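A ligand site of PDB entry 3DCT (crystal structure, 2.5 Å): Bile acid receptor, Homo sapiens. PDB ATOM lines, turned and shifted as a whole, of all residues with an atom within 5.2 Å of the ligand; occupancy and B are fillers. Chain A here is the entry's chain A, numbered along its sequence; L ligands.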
ATOM      1  N   ARG A  27     -20.500  22.720  15.303  1.00  0.00           N
ATOM      2  CA  ARG A  27     -19.935  24.054  15.520  1.00  0.00           C
ATOM      3  C   ARG A  27     -20.255  24.369  16.984  1.00  0.00           C
ATOM      4  O   ARG A  27     -20.861  23.552  17.658  1.00  0.00           O
ATOM      5  CB  ARG A  27     -20.603  25.080  14.595  1.00  0.00           C
ATOM      6  N   MET A  28     -19.842  25.528  17.499  1.00  0.00           N
ATOM      7  CA  MET A  28     -20.183  25.828  18.890  1.00  0.00           C
ATOM      8  C   MET A  28     -21.539  26.552  18.890  1.00  0.00           C
ATOM      9  O   MET A  28     -21.795  27.386  18.021  1.00  0.00           O
ATOM     10  CB  MET A  28     -19.109  26.705  19.550  1.00  0.00           C
ATOM     11  CG  MET A  28     -19.153  26.640  21.078  1.00  0.00           C
ATOM     12  SD  MET A  28     -17.957  27.701  21.921  1.00  0.00           S
ATOM     13  CE  MET A  28     -16.588  26.569  22.073  1.00  0.00           C
ATOM     14  N   THR A  33     -21.770  31.307  22.061  1.00  0.00           N
ATOM     15  CA  THR A  33     -21.025  32.333  21.358  1.00  0.00           C
ATOM     16  C   THR A  33     -21.635  33.727  21.389  1.00  0.00           C
ATOM     17  O   THR A  33     -20.918  34.705  21.226  1.00  0.00           O
ATOM     18  CB  THR A  33     -20.758  31.913  19.896  1.00  0.00           C
ATOM     19  OG1 THR A  33     -21.984  31.570  19.256  1.00  0.00           O
ATOM     20  CG2 THR A  33     -19.839  30.717  19.850  1.00  0.00           C
ATOM     21  N   ILE A  36     -20.235  36.203  24.198  1.00  0.00           N
ATOM     22  CA  ILE A  36     -18.978  36.921  24.029  1.00  0.00           C
ATOM     23  C   ILE A  36     -19.296  38.388  23.754  1.00  0.00           C
ATOM     24  O   ILE A  36     -18.536  39.289  24.110  1.00  0.00           O
ATOM     25  CB  ILE A  36     -18.174  36.366  22.837  1.00  0.00           C
ATOM     26  CG1 ILE A  36     -17.864  34.892  23.090  1.00  0.00           C
ATOM     27  CG2 ILE A  36     -16.884  37.168  22.656  1.00  0.00           C
ATOM     28  CD1 ILE A  36     -17.235  34.193  21.914  1.00  0.00           C
ATOM     29  N   PHE A  47     -14.284  34.764  32.704  1.00  0.00           N
ATOM     30  CA  PHE A  47     -13.816  33.435  33.010  1.00  0.00           C
ATOM     31  C   PHE A  47     -14.900  32.381  32.794  1.00  0.00           C
ATOM     32  O   PHE A  47     -14.632  31.319  32.250  1.00  0.00           O
ATOM     33  CB  PHE A  47     -13.325  33.405  34.456  1.00  0.00           C
ATOM     34  CG  PHE A  47     -12.918  32.046  34.919  1.00  0.00           C
ATOM     35  CD1 PHE A  47     -13.860  31.164  35.451  1.00  0.00           C
ATOM     36  CD2 PHE A  47     -11.607  31.617  34.765  1.00  0.00           C
ATOM     37  CE1 PHE A  47     -13.491  29.888  35.822  1.00  0.00           C
ATOM     38  CE2 PHE A  47     -11.224  30.347  35.116  1.00  0.00           C
ATOM     39  CZ  PHE A  47     -12.156  29.479  35.649  1.00  0.00           C
ATOM     40  N   LEU A  50     -15.460  31.703  29.066  1.00  0.00           N
ATOM     41  CA  LEU A  50     -14.325  30.940  28.575  1.00  0.00           C
ATOM     42  C   LEU A  50     -14.426  29.493  29.047  1.00  0.00           C
ATOM     43  O   LEU A  50     -14.060  28.574  28.320  1.00  0.00           O
ATOM     44  CB  LEU A  50     -13.035  31.584  29.082  1.00  0.00           C
ATOM     45  CG  LEU A  50     -12.794  32.947  28.437  1.00  0.00           C
ATOM     46  CD1 LEU A  50     -11.517  33.556  28.964  1.00  0.00           C
ATOM     47  CD2 LEU A  50     -12.728  32.758  26.931  1.00  0.00           C
ATOM     48  N   THR A  51     -14.926  29.298  30.256  1.00  0.00           N
ATOM     49  CA  THR A  51     -15.091  27.945  30.782  1.00  0.00           C
ATOM     50  C   THR A  51     -16.154  27.221  29.978  1.00  0.00           C
ATOM     51  O   THR A  51     -15.946  26.112  29.506  1.00  0.00           O
ATOM     52  CB  THR A  51     -15.518  27.958  32.247  1.00  0.00           C
ATOM     53  OG1 THR A  51     -14.448  28.463  33.035  1.00  0.00           O
ATOM     54  CG2 THR A  51     -15.839  26.545  32.718  1.00  0.00           C
ATOM     55  N   MET A  53     -17.208  27.684  26.992  1.00  0.00           N
ATOM     56  CA  MET A  53     -16.781  27.390  25.647  1.00  0.00           C
ATOM     57  C   MET A  53     -15.837  26.201  25.640  1.00  0.00           C
ATOM     58  O   MET A  53     -15.936  25.347  24.767  1.00  0.00           O
ATOM     59  CB  MET A  53     -16.114  28.595  25.038  1.00  0.00           C
ATOM     60  CG  MET A  53     -17.062  29.731  24.825  1.00  0.00           C
ATOM     61  SD  MET A  53     -16.141  31.231  24.412  1.00  0.00           S
ATOM     62  CE  MET A  53     -15.732  30.961  22.808  1.00  0.00           C
ATOM     63  N   ALA A  54     -14.933  26.153  26.610  1.00  0.00           N
ATOM     64  CA  ALA A  54     -14.004  25.036  26.656  1.00  0.00           C
ATOM     65  C   ALA A  54     -14.686  23.706  26.960  1.00  0.00           C
ATOM     66  O   ALA A  54     -14.321  22.690  26.377  1.00  0.00           O
ATOM     67  CB  ALA A  54     -12.905  25.304  27.652  1.00  0.00           C
ATOM     68  N   HIS A  57     -16.395  22.647  23.885  1.00  0.00           N
ATOM     69  CA  HIS A  57     -15.452  22.185  22.887  1.00  0.00           C
ATOM     70  C   HIS A  57     -14.855  20.818  23.202  1.00  0.00           C
ATOM     71  O   HIS A  57     -14.483  20.066  22.287  1.00  0.00           O
ATOM     72  CB  HIS A  57     -14.327  23.174  22.681  1.00  0.00           C
ATOM     73  CG  HIS A  57     -13.575  22.966  21.412  1.00  0.00           C
ATOM     74  ND1 HIS A  57     -14.130  23.206  20.175  1.00  0.00           N
ATOM     75  CD2 HIS A  57     -12.315  22.523  21.180  1.00  0.00           C
ATOM     76  CE1 HIS A  57     -13.240  22.922  19.231  1.00  0.00           C
ATOM     77  NE2 HIS A  57     -12.132  22.503  19.813  1.00  0.00           N
ATOM     78  N   VAL A  88      -5.896  20.822  25.224  1.00  0.00           N
ATOM     79  CA  VAL A  88      -5.428  22.198  25.256  1.00  0.00           C
ATOM     80  C   VAL A  88      -4.905  22.631  23.902  1.00  0.00           C
ATOM     81  O   VAL A  88      -5.187  23.733  23.446  1.00  0.00           O
ATOM     82  CB  VAL A  88      -4.325  22.424  26.296  1.00  0.00           C
ATOM     83  CG1 VAL A  88      -3.784  23.845  26.159  1.00  0.00           C
ATOM     84  CG2 VAL A  88      -4.857  22.225  27.680  1.00  0.00           C
ATOM     85  N   MET A  91      -7.582  23.146  21.402  1.00  0.00           N
ATOM     86  CA  MET A  91      -8.257  24.384  21.763  1.00  0.00           C
ATOM     87  C   MET A  91      -7.510  25.640  21.326  1.00  0.00           C
ATOM     88  O   MET A  91      -8.131  26.669  21.071  1.00  0.00           O
ATOM     89  CB  MET A  91      -8.517  24.444  23.269  1.00  0.00           C
ATOM     90  CG  MET A  91      -9.710  23.615  23.719  1.00  0.00           C
ATOM     91  SD  MET A  91      -9.957  23.601  25.506  1.00  0.00           S
ATOM     92  CE  MET A  91     -11.036  22.143  25.669  1.00  0.00           C
ATOM     93  N   PHE A  92      -6.181  25.566  21.253  1.00  0.00           N
ATOM     94  CA  PHE A  92      -5.385  26.700  20.804  1.00  0.00           C
ATOM     95  C   PHE A  92      -5.545  26.842  19.305  1.00  0.00           C
ATOM     96  O   PHE A  92      -5.576  27.952  18.781  1.00  0.00           O
ATOM     97  CB  PHE A  92      -3.900  26.501  21.067  1.00  0.00           C
ATOM     98  CG  PHE A  92      -3.390  27.230  22.257  1.00  0.00           C
ATOM     99  CD1 PHE A  92      -3.471  26.652  23.520  1.00  0.00           C
ATOM    100  CD2 PHE A  92      -2.835  28.496  22.139  1.00  0.00           C
ATOM    101  CE1 PHE A  92      -3.006  27.311  24.649  1.00  0.00           C
ATOM    102  CE2 PHE A  92      -2.367  29.169  23.254  1.00  0.00           C
ATOM    103  CZ  PHE A  92      -2.459  28.569  24.523  1.00  0.00           C
ATOM    104  N   ARG A  94      -8.193  25.798  17.509  1.00  0.00           N
ATOM    105  CA  ARG A  94      -9.547  26.263  17.215  1.00  0.00           C
ATOM    106  C   ARG A  94      -9.721  27.764  17.485  1.00  0.00           C
ATOM    107  O   ARG A  94     -10.351  28.458  16.679  1.00  0.00           O
ATOM    108  CB  ARG A  94     -10.601  25.486  18.003  1.00  0.00           C
ATOM    109  CG  ARG A  94     -12.009  25.859  17.639  1.00  0.00           C
ATOM    110  CD  ARG A  94     -12.128  26.007  16.139  1.00  0.00           C
ATOM    111  NE  ARG A  94     -13.515  26.046  15.706  1.00  0.00           N
ATOM    112  CZ  ARG A  94     -13.897  26.374  14.483  1.00  0.00           C
ATOM    113  NH1 ARG A  94     -12.989  26.685  13.572  1.00  0.00           N
ATOM    114  NH2 ARG A  94     -15.177  26.363  14.157  1.00  0.00           N
ATOM    115  N   SER A  95      -9.167  28.250  18.600  1.00  0.00           N
ATOM    116  CA  SER A  95      -9.230  29.672  18.935  1.00  0.00           C
ATOM    117  C   SER A  95      -8.390  30.485  17.927  1.00  0.00           C
ATOM    118  O   SER A  95      -8.848  31.513  17.415  1.00  0.00           O
ATOM    119  CB  SER A  95      -8.752  29.919  20.381  1.00  0.00           C
ATOM    120  OG  SER A  95      -7.518  29.307  20.641  1.00  0.00           O
ATOM    121  N   ILE A  98     -10.241  30.931  14.948  1.00  0.00           N
ATOM    122  CA  ILE A  98     -11.267  31.942  15.176  1.00  0.00           C
ATOM    123  C   ILE A  98     -10.771  33.370  14.997  1.00  0.00           C
ATOM    124  O   ILE A  98     -11.380  34.172  14.285  1.00  0.00           O
ATOM    125  CB  ILE A  98     -11.842  31.809  16.589  1.00  0.00           C
ATOM    126  CG1 ILE A  98     -12.681  30.535  16.715  1.00  0.00           C
ATOM    127  CG2 ILE A  98     -12.654  33.042  16.912  1.00  0.00           C
ATOM    128  CD1 ILE A  98     -13.820  30.453  15.739  1.00  0.00           C
ATOM    129  N   SER A 105     -19.121  34.550  14.412  1.00  0.00           N
ATOM    130  CA  SER A 105     -19.602  33.959  15.646  1.00  0.00           C
ATOM    131  C   SER A 105     -18.463  33.851  16.662  1.00  0.00           C
ATOM    132  O   SER A 105     -18.609  33.242  17.717  1.00  0.00           O
ATOM    133  CB  SER A 105     -20.181  32.567  15.372  1.00  0.00           C
ATOM    134  N   GLY A 106     -17.320  34.449  16.331  1.00  0.00           N
ATOM    135  CA  GLY A 106     -16.182  34.423  17.217  1.00  0.00           C
ATOM    136  C   GLY A 106     -15.954  35.738  17.940  1.00  0.00           C
ATOM    137  O   GLY A 106     -15.276  35.768  18.966  1.00  0.00           O
ATOM    138  N   LEU A 111     -13.800  38.702  22.203  1.00  0.00           N
ATOM    139  CA  LEU A 111     -13.328  37.441  22.729  1.00  0.00           C
ATOM    140  C   LEU A 111     -11.936  37.681  23.320  1.00  0.00           C
ATOM    141  O   LEU A 111     -11.630  37.203  24.402  1.00  0.00           O
ATOM    142  CB  LEU A 111     -13.251  36.395  21.625  1.00  0.00           C
ATOM    143  CG  LEU A 111     -12.766  35.027  22.105  1.00  0.00           C
ATOM    144  CD1 LEU A 111     -13.601  34.585  23.292  1.00  0.00           C
ATOM    145  CD2 LEU A 111     -12.887  34.021  20.984  1.00  0.00           C
ATOM    146  N   ILE A 115     -10.492  37.167  27.198  1.00  0.00           N
ATOM    147  CA  ILE A 115      -9.319  36.360  27.512  1.00  0.00           C
ATOM    148  C   ILE A 115      -8.246  37.217  28.179  1.00  0.00           C
ATOM    149  O   ILE A 115      -7.522  36.776  29.077  1.00  0.00           O
ATOM    150  CB  ILE A 115      -8.749  35.711  26.249  1.00  0.00           C
ATOM    151  CG1 ILE A 115      -9.751  34.692  25.714  1.00  0.00           C
ATOM    152  CG2 ILE A 115      -7.430  35.056  26.549  1.00  0.00           C
ATOM    153  CD1 ILE A 115      -9.356  34.074  24.401  1.00  0.00           C
ATOM    154  N   ILE A 120      -5.812  35.358  33.812  1.00  0.00           N
ATOM    155  CA  ILE A 120      -4.639  34.727  33.202  1.00  0.00           C
ATOM    156  C   ILE A 120      -3.392  35.606  33.371  1.00  0.00           C
ATOM    157  O   ILE A 120      -3.398  36.797  33.055  1.00  0.00           O
ATOM    158  CB  ILE A 120      -4.846  34.473  31.691  1.00  0.00           C
ATOM    159  CG1 ILE A 120      -6.207  33.842  31.425  1.00  0.00           C
ATOM    160  CG2 ILE A 120      -3.805  33.479  31.186  1.00  0.00           C
ATOM    161  CD1 ILE A 120      -6.387  33.419  29.992  1.00  0.00           C
ATOM    162  N   MET A 128       0.598  33.488  24.200  1.00  0.00           N
ATOM    163  CA  MET A 128      -0.660  33.047  23.629  1.00  0.00           C
ATOM    164  C   MET A 128      -1.011  33.870  22.400  1.00  0.00           C
ATOM    165  O   MET A 128      -1.322  33.336  21.344  1.00  0.00           O
ATOM    166  CB  MET A 128      -1.759  33.182  24.692  1.00  0.00           C
ATOM    167  CG  MET A 128      -3.113  32.592  24.298  1.00  0.00           C
ATOM    168  SD  MET A 128      -4.361  32.861  25.596  1.00  0.00           S
ATOM    169  CE  MET A 128      -3.641  31.961  26.931  1.00  0.00           C
ATOM    170  N   TYR A 132      -0.987  33.363  18.306  1.00  0.00           N
ATOM    171  CA  TYR A 132      -2.157  33.673  17.483  1.00  0.00           C
ATOM    172  C   TYR A 132      -1.764  34.479  16.262  1.00  0.00           C
ATOM    173  O   TYR A 132      -2.244  34.224  15.158  1.00  0.00           O
ATOM    174  CB  TYR A 132      -3.179  34.446  18.280  1.00  0.00           C
ATOM    175  CG  TYR A 132      -3.924  33.573  19.243  1.00  0.00           C
ATOM    176  CD1 TYR A 132      -4.250  32.280  18.892  1.00  0.00           C
ATOM    177  CD2 TYR A 132      -4.332  34.049  20.473  1.00  0.00           C
ATOM    178  CE1 TYR A 132      -4.977  31.476  19.729  1.00  0.00           C
ATOM    179  CE2 TYR A 132      -5.082  33.252  21.328  1.00  0.00           C
ATOM    180  CZ  TYR A 132      -5.404  31.973  20.948  1.00  0.00           C
ATOM    181  OH  TYR A 132      -6.191  31.206  21.784  1.00  0.00           O
ATOM    182  N   HIS A 210      -0.429  26.143  30.779  1.00  0.00           N
ATOM    183  CA  HIS A 210      -1.836  25.884  31.105  1.00  0.00           C
ATOM    184  C   HIS A 210      -2.062  25.204  32.458  1.00  0.00           C
ATOM    185  O   HIS A 210      -2.975  25.584  33.198  1.00  0.00           O
ATOM    186  CB  HIS A 210      -2.501  25.039  30.004  1.00  0.00           C
ATOM    187  CG  HIS A 210      -3.982  24.934  30.133  1.00  0.00           C
ATOM    188  ND1 HIS A 210      -4.602  23.898  30.802  1.00  0.00           N
ATOM    189  CD2 HIS A 210      -4.978  25.749  29.699  1.00  0.00           C
ATOM    190  CE1 HIS A 210      -5.906  24.084  30.776  1.00  0.00           C
ATOM    191  NE2 HIS A 210      -6.172  25.189  30.115  1.00  0.00           N
ATOM    192  N   TRP A 217      -5.857  29.300  39.135  1.00  0.00           N
ATOM    193  CA  TRP A 217      -7.295  29.490  39.221  1.00  0.00           C
ATOM    194  C   TRP A 217      -7.905  28.660  40.315  1.00  0.00           C
ATOM    195  O   TRP A 217      -8.836  29.102  40.973  1.00  0.00           O
ATOM    196  CB  TRP A 217      -7.924  29.087  37.909  1.00  0.00           C
ATOM    197  CG  TRP A 217      -7.858  30.093  36.836  1.00  0.00           C
ATOM    198  CD1 TRP A 217      -8.150  31.418  36.973  1.00  0.00           C
ATOM    199  CD2 TRP A 217      -7.686  29.861  35.443  1.00  0.00           C
ATOM    200  NE1 TRP A 217      -8.183  32.035  35.744  1.00  0.00           N
ATOM    201  CE2 TRP A 217      -7.900  31.093  34.786  1.00  0.00           C
ATOM    202  CE3 TRP A 217      -7.372  28.745  34.685  1.00  0.00           C
ATOM    203  CZ2 TRP A 217      -7.814  31.224  33.412  1.00  0.00           C
ATOM    204  CZ3 TRP A 217      -7.286  28.883  33.317  1.00  0.00           C
ATOM    205  CH2 TRP A 217      -7.503  30.130  32.688  1.00  0.00           C
ATOM    206  N   PHE A 224     -14.719  25.271  37.675  1.00  0.00           N
ATOM    207  CA  PHE A 224     -14.514  24.581  36.417  1.00  0.00           C
ATOM    208  C   PHE A 224     -15.688  23.671  36.229  1.00  0.00           C
ATOM    209  O   PHE A 224     -16.744  23.903  36.804  1.00  0.00           O
ATOM    210  CB  PHE A 224     -13.247  23.732  36.465  1.00  0.00           C
ATOM    211  CG  PHE A 224     -11.990  24.543  36.387  1.00  0.00           C
ATOM    212  CD1 PHE A 224     -11.030  24.446  37.387  1.00  0.00           C
ATOM    213  CD2 PHE A 224     -11.786  25.405  35.319  1.00  0.00           C
ATOM    214  CE1 PHE A 224      -9.895  25.225  37.315  1.00  0.00           C
ATOM    215  CE2 PHE A 224     -10.652  26.170  35.248  1.00  0.00           C
ATOM    216  CZ  PHE A 224      -9.701  26.094  36.239  1.00  0.00           C
ATOM    217  N   LEU A 228     -14.098  19.263  32.417  1.00  0.00           N
ATOM    218  CA  LEU A 228     -12.783  19.889  32.321  1.00  0.00           C
ATOM    219  C   LEU A 228     -11.851  19.383  33.397  1.00  0.00           C
ATOM    220  O   LEU A 228     -10.663  19.224  33.151  1.00  0.00           O
ATOM    221  CB  LEU A 228     -12.913  21.407  32.404  1.00  0.00           C
ATOM    222  CG  LEU A 228     -13.530  22.052  31.173  1.00  0.00           C
ATOM    223  CD1 LEU A 228     -13.648  23.544  31.400  1.00  0.00           C
ATOM    224  CD2 LEU A 228     -12.666  21.736  29.955  1.00  0.00           C
ATOM    225  N   TRP A 232      -8.374  17.428  32.527  1.00  0.00           N
ATOM    226  CA  TRP A 232      -7.167  18.087  32.980  1.00  0.00           C
ATOM    227  C   TRP A 232      -6.726  17.725  34.375  1.00  0.00           C
ATOM    228  O   TRP A 232      -6.078  18.528  35.040  1.00  0.00           O
ATOM    229  CB  TRP A 232      -7.335  19.582  32.879  1.00  0.00           C
ATOM    230  CG  TRP A 232      -7.407  20.048  31.457  1.00  0.00           C
ATOM    231  CD1 TRP A 232      -6.813  19.437  30.403  1.00  0.00           C
ATOM    232  CD2 TRP A 232      -8.044  21.207  30.948  1.00  0.00           C
ATOM    233  NE1 TRP A 232      -7.045  20.144  29.248  1.00  0.00           N
ATOM    234  CE2 TRP A 232      -7.807  21.242  29.558  1.00  0.00           C
ATOM    235  CE3 TRP A 232      -8.790  22.217  31.511  1.00  0.00           C
ATOM    236  CZ2 TRP A 232      -8.289  22.244  28.751  1.00  0.00           C
ATOM    237  CZ3 TRP A 232      -9.270  23.219  30.689  1.00  0.00           C
ATOM    238  CH2 TRP A 232      -9.015  23.218  29.310  1.00  0.00           C
HETATM  239  C1  LIG L   1      -8.317  28.425  28.163  1.00  0.00           C
HETATM  240  N1  LIG L   1      -7.806  28.307  29.442  1.00  0.00           N
HETATM  241  C2  LIG L   1      -9.948  28.438  29.661  1.00  0.00           C
HETATM  242  C3  LIG L   1     -10.825  28.630  27.223  1.00  0.00           C
HETATM  243  C4  LIG L   1      -7.286  29.758  26.371  1.00  0.00           C
HETATM  244  C5  LIG L   1      -7.083  27.249  26.346  1.00  0.00           C
HETATM  245  C6  LIG L   1     -11.309  28.517  30.393  1.00  0.00           C
HETATM  246  C7  LIG L   1     -11.720  27.143  31.017  1.00  0.00           C
HETATM  247  C8  LIG L   1     -11.246  29.574  31.500  1.00  0.00           C
HETATM  248  C9  LIG L   1     -11.412  27.813  24.955  1.00  0.00           C
HETATM  249  C10 LIG L   1      -6.081  28.646  24.556  1.00  0.00           C
HETATM  250  C11 LIG L   1     -11.603  26.790  23.988  1.00  0.00           C
HETATM  251  C12 LIG L   1     -11.842  29.177  24.674  1.00  0.00           C
HETATM  252  C13 LIG L   1     -12.240  27.082  22.776  1.00  0.00           C
HETATM  253  C14 LIG L   1     -12.495  29.482  23.431  1.00  0.00           C
HETATM  254  C15 LIG L   1     -12.667  28.409  22.461  1.00  0.00           C
HETATM  255  C16 LIG L   1     -13.352  28.559  21.131  1.00  0.00           C
HETATM  256  C17 LIG L   1     -14.410  29.273  20.927  1.00  0.00           C
HETATM  257  C18 LIG L   1     -15.262  29.357  19.705  1.00  0.00           C
HETATM  258  C19 LIG L   1     -15.464  28.162  19.033  1.00  0.00           C
HETATM  259  C20 LIG L   1     -15.906  30.581  19.258  1.00  0.00           C
HETATM  260  C21 LIG L   1     -16.726  30.503  18.080  1.00  0.00           C
HETATM  261  C22 LIG L   1      -9.713  28.495  28.292  1.00  0.00           C
HETATM  262  C23 LIG L   1      -7.591  28.466  26.978  1.00  0.00           C
HETATM  263  O1  LIG L   1      -8.746  28.315  30.335  1.00  0.00           O
HETATM  264  O2  LIG L   1     -10.819  27.566  26.203  1.00  0.00           O
HETATM  265  C24 LIG L   1      -6.547  29.834  25.166  1.00  0.00           C
HETATM  266 CL1  LIG L   1      -7.852  31.310  27.039  1.00  0.00          CL
HETATM  267  C25 LIG L   1      -6.363  27.354  25.137  1.00  0.00           C
HETATM  268 CL2  LIG L   1      -7.365  25.617  26.948  1.00  0.00          CL
HETATM  269 CL3  LIG L   1     -12.426  25.780  21.637  1.00  0.00          CL
HETATM  270  C26 LIG L   1     -16.259  28.069  17.887  1.00  0.00           C
HETATM  271  C27 LIG L   1     -16.898  29.250  17.398  1.00  0.00           C
HETATM  272  C28 LIG L   1     -16.460  26.733  17.189  1.00  0.00           C
HETATM  273  O3  LIG L   1     -17.249  26.676  16.078  1.00  0.00           O
HETATM  274  O4  LIG L   1     -15.933  25.688  17.625  1.00  0.00           O
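Residues that only touch the ligand: Met 53, His 57, Trp 217, Ser 105, Phe 92, Ala 54, His 210, Leu 50, Thr 51, Met 91, Thr 33, Tyr 132, Phe 47, Ile 98, Trp 232, Met 128, Arg 27, Ile 115 and Ile 120.
Hydrophobic or aromatic side chains that line the ligand: Met 28, Phe 47, Leu 50, Met 53, Ala 54, His 57, Met 91, Phe 92, Ile 98, Ile 115, Ile 120, Met 128, His 210, Trp 217 and Trp 232.
The guanidinium group of Arg 94 is in salt-bridge range of an oxygen (O3) of the ligand (2.8 Å).
O3 of the ligand is in hydrogen-bond range of N of Met 28 (3.2 Å).
O of Phe 92 sits at hydrogen-bond distance from OG of Ser 95, 3.0 Å away.
The backbone carbonyl oxygen (O) of Phe 47 is in hydrogen-bond range of the side-chain hydroxyl (OG1) of Thr 51 (3.0 Å).
The backbone carbonyl oxygen of Met 91 is in hydrogen-bond range of the side-chain hydroxyl of Ser 95 (2.7 Å).
The side-chain hydroxyl (OG) of Ser 95 lies within hydrogen-bond range of the side-chain hydroxyl (OH) of Tyr 132, at 2.6 Å.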
